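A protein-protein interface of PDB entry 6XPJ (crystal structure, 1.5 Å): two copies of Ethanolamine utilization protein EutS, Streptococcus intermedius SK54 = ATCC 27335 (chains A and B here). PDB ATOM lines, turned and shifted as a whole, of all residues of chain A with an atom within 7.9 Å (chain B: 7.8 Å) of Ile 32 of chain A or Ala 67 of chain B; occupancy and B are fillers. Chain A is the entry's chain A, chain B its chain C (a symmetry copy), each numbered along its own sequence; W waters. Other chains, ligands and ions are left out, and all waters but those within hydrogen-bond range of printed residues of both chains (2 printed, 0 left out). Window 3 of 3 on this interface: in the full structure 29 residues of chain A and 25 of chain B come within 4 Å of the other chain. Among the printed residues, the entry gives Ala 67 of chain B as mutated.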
ATOM      1  N   ILE A  28     -13.173   3.233 -23.297  1.00  0.00           N
ATOM      2  CA  ILE A  28     -13.279   4.484 -24.085  1.00  0.00           C
ATOM      3  C   ILE A  28     -12.994   4.051 -25.516  1.00  0.00           C
ATOM      4  O   ILE A  28     -11.845   3.658 -25.803  1.00  0.00           O
ATOM      5  CB  ILE A  28     -12.321   5.577 -23.573  1.00  0.00           C
ATOM      6  CG1 ILE A  28     -12.483   5.813 -22.068  1.00  0.00           C
ATOM      7  CG2 ILE A  28     -12.532   6.870 -24.370  1.00  0.00           C
ATOM      8  CD1 ILE A  28     -11.495   6.830 -21.518  1.00  0.00           C
ATOM      9  N   ALA A  29     -14.013   4.047 -26.372  1.00  0.00           N
ATOM     10  CA  ALA A  29     -13.936   3.401 -27.702  1.00  0.00           C
ATOM     11  C   ALA A  29     -12.976   4.167 -28.606  1.00  0.00           C
ATOM     12  O   ALA A  29     -12.163   3.503 -29.326  1.00  0.00           O
ATOM     13  CB  ALA A  29     -15.313   3.322 -28.320  1.00  0.00           C
ATOM     14  N   ALA A  30     -13.042   5.505 -28.572  1.00  0.00           N
ATOM     15  CA  ALA A  30     -12.274   6.392 -29.472  1.00  0.00           C
ATOM     16  C   ALA A  30     -11.750   7.571 -28.666  1.00  0.00           C
ATOM     17  O   ALA A  30     -12.243   8.688 -28.809  1.00  0.00           O
ATOM     18  CB  ALA A  30     -13.160   6.815 -30.625  1.00  0.00           C
ATOM     19  N   PRO A  31     -10.733   7.365 -27.800  1.00  0.00           N
ATOM     20  CA  PRO A  31     -10.219   8.444 -26.960  1.00  0.00           C
ATOM     21  C   PRO A  31      -9.822   9.685 -27.768  1.00  0.00           C
ATOM     22  O   PRO A  31      -9.283   9.572 -28.871  1.00  0.00           O
ATOM     23  CB  PRO A  31      -8.995   7.840 -26.271  1.00  0.00           C
ATOM     24  CG  PRO A  31      -9.268   6.348 -26.287  1.00  0.00           C
ATOM     25  CD  PRO A  31     -10.036   6.083 -27.557  1.00  0.00           C
ATOM     26  N   ILE A  32     -10.025  10.841 -27.161  1.00  0.00           N
ATOM     27  CA  ILE A  32      -9.427  12.114 -27.655  1.00  0.00           C
ATOM     28  C   ILE A  32      -7.903  12.093 -27.471  1.00  0.00           C
ATOM     29  O   ILE A  32      -7.368  11.348 -26.621  1.00  0.00           O
ATOM     30  CB  ILE A  32     -10.085  13.327 -26.979  1.00  0.00           C
ATOM     31  CG1 ILE A  32      -9.738  13.402 -25.494  1.00  0.00           C
ATOM     32  CG2 ILE A  32     -11.584  13.300 -27.249  1.00  0.00           C
ATOM     33  CD1 ILE A  32     -10.182  14.669 -24.813  1.00  0.00           C
ATOM     34  N   GLU A  33      -7.224  12.951 -28.226  1.00  0.00           N
ATOM     35  CA  GLU A  33      -5.737  13.014 -28.256  1.00  0.00           C
ATOM     36  C   GLU A  33      -5.169  13.269 -26.857  1.00  0.00           C
ATOM     37  O   GLU A  33      -4.185  12.609 -26.491  1.00  0.00           O
ATOM     38  CB  GLU A  33      -5.310  14.085 -29.263  1.00  0.00           C
ATOM     39  CG  GLU A  33      -5.602  13.673 -30.687  1.00  0.00           C
ATOM     40  CD  GLU A  33      -4.827  12.445 -31.146  1.00  0.00           C
ATOM     41  OE1 GLU A  33      -3.610  12.580 -31.377  1.00  0.00           O
ATOM     42  OE2 GLU A  33      -5.434  11.354 -31.255  1.00  0.00           O
ATOM     43  N   ALA A  34      -5.769  14.183 -26.078  1.00  0.00           N
ATOM     44  CA  ALA A  34      -5.255  14.575 -24.741  1.00  0.00           C
ATOM     45  C   ALA A  34      -5.232  13.359 -23.814  1.00  0.00           C
ATOM     46  O   ALA A  34      -4.377  13.261 -22.931  1.00  0.00           O
ATOM     47  CB  ALA A  34      -6.084  15.708 -24.173  1.00  0.00           C
ATOM     48  N   VAL A  35      -6.157  12.422 -24.012  1.00  0.00           N
ATOM     49  CA  VAL A  35      -6.290  11.230 -23.136  1.00  0.00           C
ATOM     50  C   VAL A  35      -5.213  10.205 -23.498  1.00  0.00           C
ATOM     51  O   VAL A  35      -4.595   9.594 -22.613  1.00  0.00           O
ATOM     52  CB  VAL A  35      -7.728  10.683 -23.250  1.00  0.00           C
ATOM     53  CG1 VAL A  35      -7.822   9.229 -22.851  1.00  0.00           C
ATOM     54  CG2 VAL A  35      -8.671  11.552 -22.441  1.00  0.00           C
ATOM     55  N   TYR A  36      -4.984   9.976 -24.787  1.00  0.00           N
ATOM     56  CA  TYR A  36      -3.841   9.127 -25.178  1.00  0.00           C
ATOM     57  C   TYR A  36      -2.560   9.744 -24.594  1.00  0.00           C
ATOM     58  O   TYR A  36      -1.725   9.030 -24.055  1.00  0.00           O
ATOM     59  CB  TYR A  36      -3.743   9.061 -26.693  1.00  0.00           C
ATOM     60  CG  TYR A  36      -4.764   8.245 -27.444  1.00  0.00           C
ATOM     61  CD1 TYR A  36      -5.012   6.917 -27.129  1.00  0.00           C
ATOM     62  CD2 TYR A  36      -5.392   8.777 -28.553  1.00  0.00           C
ATOM     63  CE1 TYR A  36      -5.874   6.160 -27.901  1.00  0.00           C
ATOM     64  CE2 TYR A  36      -6.237   8.028 -29.349  1.00  0.00           C
ATOM     65  CZ  TYR A  36      -6.480   6.712 -29.020  1.00  0.00           C
ATOM     66  OH  TYR A  36      -7.309   6.009 -29.841  1.00  0.00           O
ATOM     67  N   GLU A  37      -2.427  11.071 -24.700  1.00  0.00           N
ATOM     68  CA  GLU A  37      -1.178  11.772 -24.283  1.00  0.00           C
ATOM     69  C   GLU A  37      -1.007  11.632 -22.759  1.00  0.00           C
ATOM     70  O   GLU A  37       0.114  11.349 -22.329  1.00  0.00           O
ATOM     71  CB  GLU A  37      -1.141  13.209 -24.812  1.00  0.00           C
ATOM     72  CG  GLU A  37       0.266  13.802 -24.889  1.00  0.00           C
ATOM     73  CD  GLU A  37       1.200  13.294 -25.989  1.00  0.00           C
ATOM     74  OE1 GLU A  37       0.718  12.953 -27.081  1.00  0.00           O
ATOM     75  OE2 GLU A  37       2.428  13.261 -25.758  1.00  0.00           O
ATOM     76  N   CYS A  38      -2.071  11.733 -21.955  1.00  0.00           N
ATOM     77  CA  CYS A  38      -1.960  11.635 -20.474  1.00  0.00           C
ATOM     78  C   CYS A  38      -1.484  10.228 -20.068  1.00  0.00           C
ATOM     79  O   CYS A  38      -0.777  10.141 -19.063  1.00  0.00           O
ATOM     80  CB  CYS A  38      -3.255  12.058 -19.774  1.00  0.00           C
ATOM     81  SG  CYS A  38      -4.328  10.673 -19.316  1.00  0.00           S
ATOM     82  N   HIS A  43      -1.466   6.761 -30.117  1.00  0.00           N
ATOM     83  CA  HIS A  43      -2.791   7.413 -30.322  1.00  0.00           C
ATOM     84  C   HIS A  43      -3.626   6.567 -31.291  1.00  0.00           C
ATOM     85  O   HIS A  43      -4.006   7.044 -32.353  1.00  0.00           O
ATOM     86  CB  HIS A  43      -2.656   8.859 -30.785  1.00  0.00           C
ATOM     87  CG  HIS A  43      -1.904   9.730 -29.851  1.00  0.00           C
ATOM     88  ND1 HIS A  43      -2.001  11.096 -29.913  1.00  0.00           N
ATOM     89  CD2 HIS A  43      -1.035   9.467 -28.852  1.00  0.00           C
ATOM     90  CE1 HIS A  43      -1.244  11.636 -28.988  1.00  0.00           C
ATOM     91  NE2 HIS A  43      -0.648  10.653 -28.315  1.00  0.00           N
ATOM     92  N   GLY A  45      -6.688   3.117 -31.173  1.00  0.00           N
ATOM     93  CA  GLY A  45      -7.443   2.072 -30.485  1.00  0.00           C
ATOM     94  C   GLY A  45      -8.144   2.570 -29.238  1.00  0.00           C
ATOM     95  O   GLY A  45      -8.130   3.775 -28.936  1.00  0.00           O
ATOM     96  N   ILE A  47      -9.282   2.261 -25.062  1.00  0.00           N
ATOM     97  CA  ILE A  47      -8.648   2.146 -23.733  1.00  0.00           C
ATOM     98  C   ILE A  47      -9.630   1.446 -22.807  1.00  0.00           C
ATOM     99  O   ILE A  47     -10.769   1.909 -22.701  1.00  0.00           O
ATOM    100  CB  ILE A  47      -8.253   3.533 -23.211  1.00  0.00           C
ATOM    101  CG1 ILE A  47      -7.132   4.126 -24.067  1.00  0.00           C
ATOM    102  CG2 ILE A  47      -7.842   3.462 -21.740  1.00  0.00           C
ATOM    103  CD1 ILE A  47      -5.801   3.436 -23.891  1.00  0.00           C
ATOM    104  N   SER A 117     -17.807   4.573 -23.284  1.00  0.00           N
ATOM    105  CA  SER A 117     -17.868   5.975 -23.753  1.00  0.00           C
ATOM    106  C   SER A 117     -17.053   6.118 -25.034  1.00  0.00           C
ATOM    107  O   SER A 117     -16.540   5.157 -25.578  1.00  0.00           O
ATOM    108  CB  SER A 117     -17.430   6.898 -22.671  1.00  0.00           C
ATOM    109  OG  SER A 117     -16.064   6.680 -22.318  1.00  0.00           O
ATOM    110  OXT SER A 117     -16.973   7.271 -25.493  1.00  0.00           O
ATOM    111  N   ILE B  59     -10.243   9.798 -15.992  1.00  0.00           N
ATOM    112  CA  ILE B  59      -9.879   9.752 -17.438  1.00  0.00           C
ATOM    113  C   ILE B  59     -11.147   9.752 -18.314  1.00  0.00           C
ATOM    114  O   ILE B  59     -11.129  10.362 -19.386  1.00  0.00           O
ATOM    115  CB  ILE B  59      -8.955   8.565 -17.732  1.00  0.00           C
ATOM    116  CG1 ILE B  59      -8.324   8.671 -19.119  1.00  0.00           C
ATOM    117  CG2 ILE B  59      -9.685   7.260 -17.589  1.00  0.00           C
ATOM    118  CD1 ILE B  59      -7.378   9.852 -19.267  1.00  0.00           C
ATOM    119  N   ILE B  60     -12.238   9.150 -17.855  1.00  0.00           N
ATOM    120  CA  ILE B  60     -13.498   9.112 -18.624  1.00  0.00           C
ATOM    121  C   ILE B  60     -14.060  10.531 -18.692  1.00  0.00           C
ATOM    122  O   ILE B  60     -14.485  10.976 -19.765  1.00  0.00           O
ATOM    123  CB  ILE B  60     -14.497   8.159 -17.942  1.00  0.00           C
ATOM    124  CG1 ILE B  60     -13.965   6.743 -17.868  1.00  0.00           C
ATOM    125  CG2 ILE B  60     -15.843   8.222 -18.638  1.00  0.00           C
ATOM    126  CD1 ILE B  60     -14.801   5.826 -16.980  1.00  0.00           C
ATOM    127  N   ALA B  61     -14.061  11.247 -17.574  1.00  0.00           N
ATOM    128  CA  ALA B  61     -14.588  12.629 -17.500  1.00  0.00           C
ATOM    129  C   ALA B  61     -13.731  13.554 -18.349  1.00  0.00           C
ATOM    130  O   ALA B  61     -14.296  14.375 -19.073  1.00  0.00           O
ATOM    131  CB  ALA B  61     -14.676  13.117 -16.083  1.00  0.00           C
ATOM    132  N   ALA B  62     -12.417  13.379 -18.362  1.00  0.00           N
ATOM    133  CA  ALA B  62     -11.515  14.223 -19.173  1.00  0.00           C
ATOM    134  C   ALA B  62     -11.817  14.009 -20.652  1.00  0.00           C
ATOM    135  O   ALA B  62     -11.884  14.995 -21.422  1.00  0.00           O
ATOM    136  CB  ALA B  62     -10.081  13.900 -18.874  1.00  0.00           C
ATOM    137  N   ASP B  63     -12.032  12.763 -21.039  1.00  0.00           N
ATOM    138  CA  ASP B  63     -12.340  12.444 -22.454  1.00  0.00           C
ATOM    139  C   ASP B  63     -13.647  13.120 -22.878  1.00  0.00           C
ATOM    140  O   ASP B  63     -13.729  13.712 -24.001  1.00  0.00           O
ATOM    141  CB  ASP B  63     -12.396  10.936 -22.642  1.00  0.00           C
ATOM    142  CG  ASP B  63     -12.715  10.558 -24.069  1.00  0.00           C
ATOM    143  OD1 ASP B  63     -11.767  10.591 -24.881  1.00  0.00           O
ATOM    144  OD2 ASP B  63     -13.860  10.220 -24.339  1.00  0.00           O
ATOM    145  N   ILE B  64     -14.691  13.010 -22.066  1.00  0.00           N
ATOM    146  CA  ILE B  64     -15.989  13.657 -22.378  1.00  0.00           C
ATOM    147  C   ILE B  64     -15.772  15.159 -22.466  1.00  0.00           C
ATOM    148  O   ILE B  64     -16.301  15.787 -23.417  1.00  0.00           O
ATOM    149  CB  ILE B  64     -17.039  13.264 -21.340  1.00  0.00           C
ATOM    150  CG1 ILE B  64     -17.374  11.789 -21.437  1.00  0.00           C
ATOM    151  CG2 ILE B  64     -18.299  14.140 -21.455  1.00  0.00           C
ATOM    152  CD1 ILE B  64     -18.081  11.284 -20.238  1.00  0.00           C
ATOM    153  N   ALA B  65     -15.081  15.761 -21.501  1.00  0.00           N
ATOM    154  CA  ALA B  65     -14.886  17.225 -21.459  1.00  0.00           C
ATOM    155  C   ALA B  65     -14.254  17.689 -22.762  1.00  0.00           C
ATOM    156  O   ALA B  65     -14.800  18.616 -23.378  1.00  0.00           O
ATOM    157  CB  ALA B  65     -14.072  17.653 -20.268  1.00  0.00           C
ATOM    158  N   GLY B  66     -13.145  17.072 -23.166  1.00  0.00           N
ATOM    159  CA  GLY B  66     -12.396  17.467 -24.377  1.00  0.00           C
ATOM    160  C   GLY B  66     -13.164  17.201 -25.652  1.00  0.00           C
ATOM    161  O   GLY B  66     -13.015  18.006 -26.631  1.00  0.00           O
ATOM    162  N   ALA B  67     -14.031  16.193 -25.674  1.00  0.00           N
ATOM    163  CA  ALA B  67     -14.855  15.872 -26.872  1.00  0.00           C
ATOM    164  C   ALA B  67     -16.036  16.858 -26.964  1.00  0.00           C
ATOM    165  O   ALA B  67     -16.551  17.052 -28.087  1.00  0.00           O
ATOM    166  CB  ALA B  67     -15.346  14.457 -26.846  1.00  0.00           C
ATOM    167  N   ALA B  68     -16.485  17.426 -25.835  1.00  0.00           N
ATOM    168  CA  ALA B  68     -17.755  18.197 -25.722  1.00  0.00           C
ATOM    169  C   ALA B  68     -17.610  19.625 -26.265  1.00  0.00           C
ATOM    170  O   ALA B  68     -18.633  20.209 -26.737  1.00  0.00           O
ATOM    171  CB  ALA B  68     -18.203  18.231 -24.277  1.00  0.00           C
ATOM    172  N   ALA B  69     -16.435  20.228 -26.123  1.00  0.00           N
ATOM    173  CA  ALA B  69     -16.243  21.677 -26.326  1.00  0.00           C
ATOM    174  C   ALA B  69     -14.756  21.938 -26.489  1.00  0.00           C
ATOM    175  O   ALA B  69     -13.965  21.021 -26.190  1.00  0.00           O
ATOM    176  CB  ALA B  69     -16.791  22.432 -25.136  1.00  0.00           C
ATOM    177  N   ASN B  70     -14.413  23.147 -26.922  1.00  0.00           N
ATOM    178  CA  ASN B  70     -13.010  23.581 -27.117  1.00  0.00           C
ATOM    179  C   ASN B  70     -12.429  23.992 -25.760  1.00  0.00           C
ATOM    180  O   ASN B  70     -12.428  25.177 -25.409  1.00  0.00           O
ATOM    181  CB  ASN B  70     -12.918  24.729 -28.113  1.00  0.00           C
ATOM    182  CG  ASN B  70     -11.491  25.164 -28.356  1.00  0.00           C
ATOM    183  OD1 ASN B  70     -10.549  24.443 -28.021  1.00  0.00           O
ATOM    184  ND2 ASN B  70     -11.327  26.350 -28.918  1.00  0.00           N
ATOM    185  N   ILE B  71     -11.937  23.022 -25.029  1.00  0.00           N
ATOM    186  CA  ILE B  71     -11.328  23.245 -23.697  1.00  0.00           C
ATOM    187  C   ILE B  71      -9.897  22.712 -23.775  1.00  0.00           C
ATOM    188  O   ILE B  71      -9.565  21.917 -24.688  1.00  0.00           O
ATOM    189  CB  ILE B  71     -12.180  22.633 -22.557  1.00  0.00           C
ATOM    190  CG1 ILE B  71     -12.412  21.132 -22.725  1.00  0.00           C
ATOM    191  CG2 ILE B  71     -13.503  23.391 -22.379  1.00  0.00           C
ATOM    192  CD1 ILE B  71     -11.415  20.271 -22.031  1.00  0.00           C
ATOM    193  N   ILE B  73      -7.324  20.660 -21.316  1.00  0.00           N
ATOM    194  CA  ILE B  73      -7.203  19.863 -20.071  1.00  0.00           C
ATOM    195  C   ILE B  73      -5.990  20.388 -19.299  1.00  0.00           C
ATOM    196  O   ILE B  73      -4.876  20.442 -19.870  1.00  0.00           O
ATOM    197  CB  ILE B  73      -7.115  18.358 -20.360  1.00  0.00           C
ATOM    198  CG1 ILE B  73      -8.365  17.826 -21.064  1.00  0.00           C
ATOM    199  CG2 ILE B  73      -6.835  17.612 -19.061  1.00  0.00           C
ATOM    200  CD1 ILE B  73      -9.566  17.680 -20.163  1.00  0.00           C
ATOM    201  N   THR B  94     -20.367  23.803 -20.986  1.00  0.00           N
ATOM    202  CA  THR B  94     -20.814  22.727 -21.895  1.00  0.00           C
ATOM    203  C   THR B  94     -20.127  21.426 -21.490  1.00  0.00           C
ATOM    204  O   THR B  94     -20.792  20.390 -21.380  1.00  0.00           O
ATOM    205  CB  THR B  94     -20.543  23.064 -23.366  1.00  0.00           C
ATOM    206  OG1 THR B  94     -21.387  24.184 -23.649  1.00  0.00           O
ATOM    207  CG2 THR B  94     -20.822  21.906 -24.299  1.00  0.00           C
ATOM    208  N   SER B  95     -18.813  21.473 -21.261  1.00  0.00           N
ATOM    209  CA  SER B  95     -18.040  20.267 -20.900  1.00  0.00           C
ATOM    210  C   SER B  95     -18.530  19.714 -19.552  1.00  0.00           C
ATOM    211  O   SER B  95     -18.674  18.508 -19.417  1.00  0.00           O
ATOM    212  CB  SER B  95     -16.564  20.547 -20.876  1.00  0.00           C
ATOM    213  OG  SER B  95     -16.078  20.782 -22.204  1.00  0.00           O
ATOM    214  N   ASP B  98     -21.881  18.065 -20.041  1.00  0.00           N
ATOM    215  CA  ASP B  98     -21.790  16.788 -20.783  1.00  0.00           C
ATOM    216  C   ASP B  98     -21.257  15.705 -19.852  1.00  0.00           C
ATOM    217  O   ASP B  98     -21.738  14.555 -19.906  1.00  0.00           O
ATOM    218  CB  ASP B  98     -20.982  16.960 -22.064  1.00  0.00           C
ATOM    219  CG  ASP B  98     -21.781  17.691 -23.145  1.00  0.00           C
ATOM    220  OD1 ASP B  98     -22.859  18.229 -22.843  1.00  0.00           O
ATOM    221  OD2 ASP B  98     -21.360  17.620 -24.304  1.00  0.00           O
HETATM  222  O   HOH W   1     -13.954  10.000 -27.044  1.00  0.00           O
HETATM  223  O   HOH W   2     -14.984   9.085 -21.982  1.00  0.00           O
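The backbone NH of Ile 32 of chain A sits at hydrogen-bond distance from the side-chain carboxylate of Asp 63 of chain B (2.9 Å).
The backbone NH (N) of Ile 28 of chain A is in hydrogen-bond range of the backbone carbonyl oxygen (O) of Ile 47 of chain A, at 2.8 Å. N of Ala 29 of chain A lies within hydrogen-bond range of O of Ser 117 of chain A, at 2.9 Å. O of Val 35 of chain A is in hydrogen-bond range of SG of Cys 38 of chain A (3.5 Å).
Among the printed residues, pairs that only touch across the chains: Cys 38 of chain A with Ile 59 of chain B (3.2 Å), Pro 31 of chain A with Asp 63 of chain B (3.4 Å), Ile 32 of chain A with Gly 66 of chain B (3.6 Å), Ile 28 of chain A with Asp 63 of chain B (3.6 Å), Val 35 of chain A with Ile 59 of chain B (3.7 Å), Val 35 of chain A with Asp 63 of chain B (3.8 Å), Ile 32 of chain A with Ala 62 of chain B (3.8 Å), Ile 32 of chain A with Ala 67 of chain B (3.96 Å) and Ser 117 of chain A with Ile 60 of chain B (3.996 Å).
Of chain B, only Ala 62 (3.8 Å), Asp 63 (2.9 Å), Gly 66 (3.6 Å) and Ala 67 (3.96 Å) come within 4 Å of Ile 32 of chain A. Printed residues of chain A within 4 Å of Ala 67 of chain B: Ile 32. Of the printed residues of chain A, Ile 60 of chain B touches Ser 117. Of the printed residues of chain B, Cys 38 of chain A touches Ile 59. Printed residues of chain B within 4 Å of Val 35 of chain A: Ile 59 and Asp 63. Of the printed residues of chain B, Ser 117 of chain A touches Ile 60 (3.996 Å). Of the printed residues of chain A, Asp 63 of chain B touches Ile 28 (3.6 Å), Pro 31 (3.4 Å), Ile 32 (2.9 Å) and Val 35 (3.8 Å). Ala 69 of chain B touches none of the printed residues of chain A. The nearest residue of chain B that does not touch Ile 32 of chain A is Ile 73 of chain B (5.2 Å). The nearest residue of chain A that does not touch Ala 67 of chain B is Ala 30 of chain A (6.8 Å). The nearest printed residue of chain B that does not touch Val 35 of chain A is Ala 62 of chain B (4.4 Å).
Of the 17 printed residues of chain B, 6 touch a printed residue of chain A. Hydrophobic or aromatic side chains of chain B that line the printed part of chain A: Ile 59, Ile 60 and Ala 67. Of the 15 printed residues of chain A, 6 touch a printed residue of chain B. Printed residues of chain A that touch a printed residue of chain B: Ile 28, Pro 31, Ile 32, Val 35, Cys 38 and Ser 117. Hydrophobic or aromatic side chains of chain A within 4 Å of the printed part of chain B: Ile 28, Ile 32 and Val 35. Among the printed residues, no Asp or Glu carboxylate lies within 4 Å of a Lys or Arg side-chain nitrogen of the other chain.
No position is printed for both chains.
Water W2 lies within hydrogen-bond range of OG of Ser 117 of chain A (2.7 Å), OD2 of Asp 63 of chain B (2.8 Å) and O of Ile 60 of chain B (3.0 Å). Water W1 lies within hydrogen-bond range of the side-chain carboxylate of Asp 63 of chain B (2.7 Å) and the backbone carbonyl oxygen of Ala 30 of chain A (2.8 Å).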
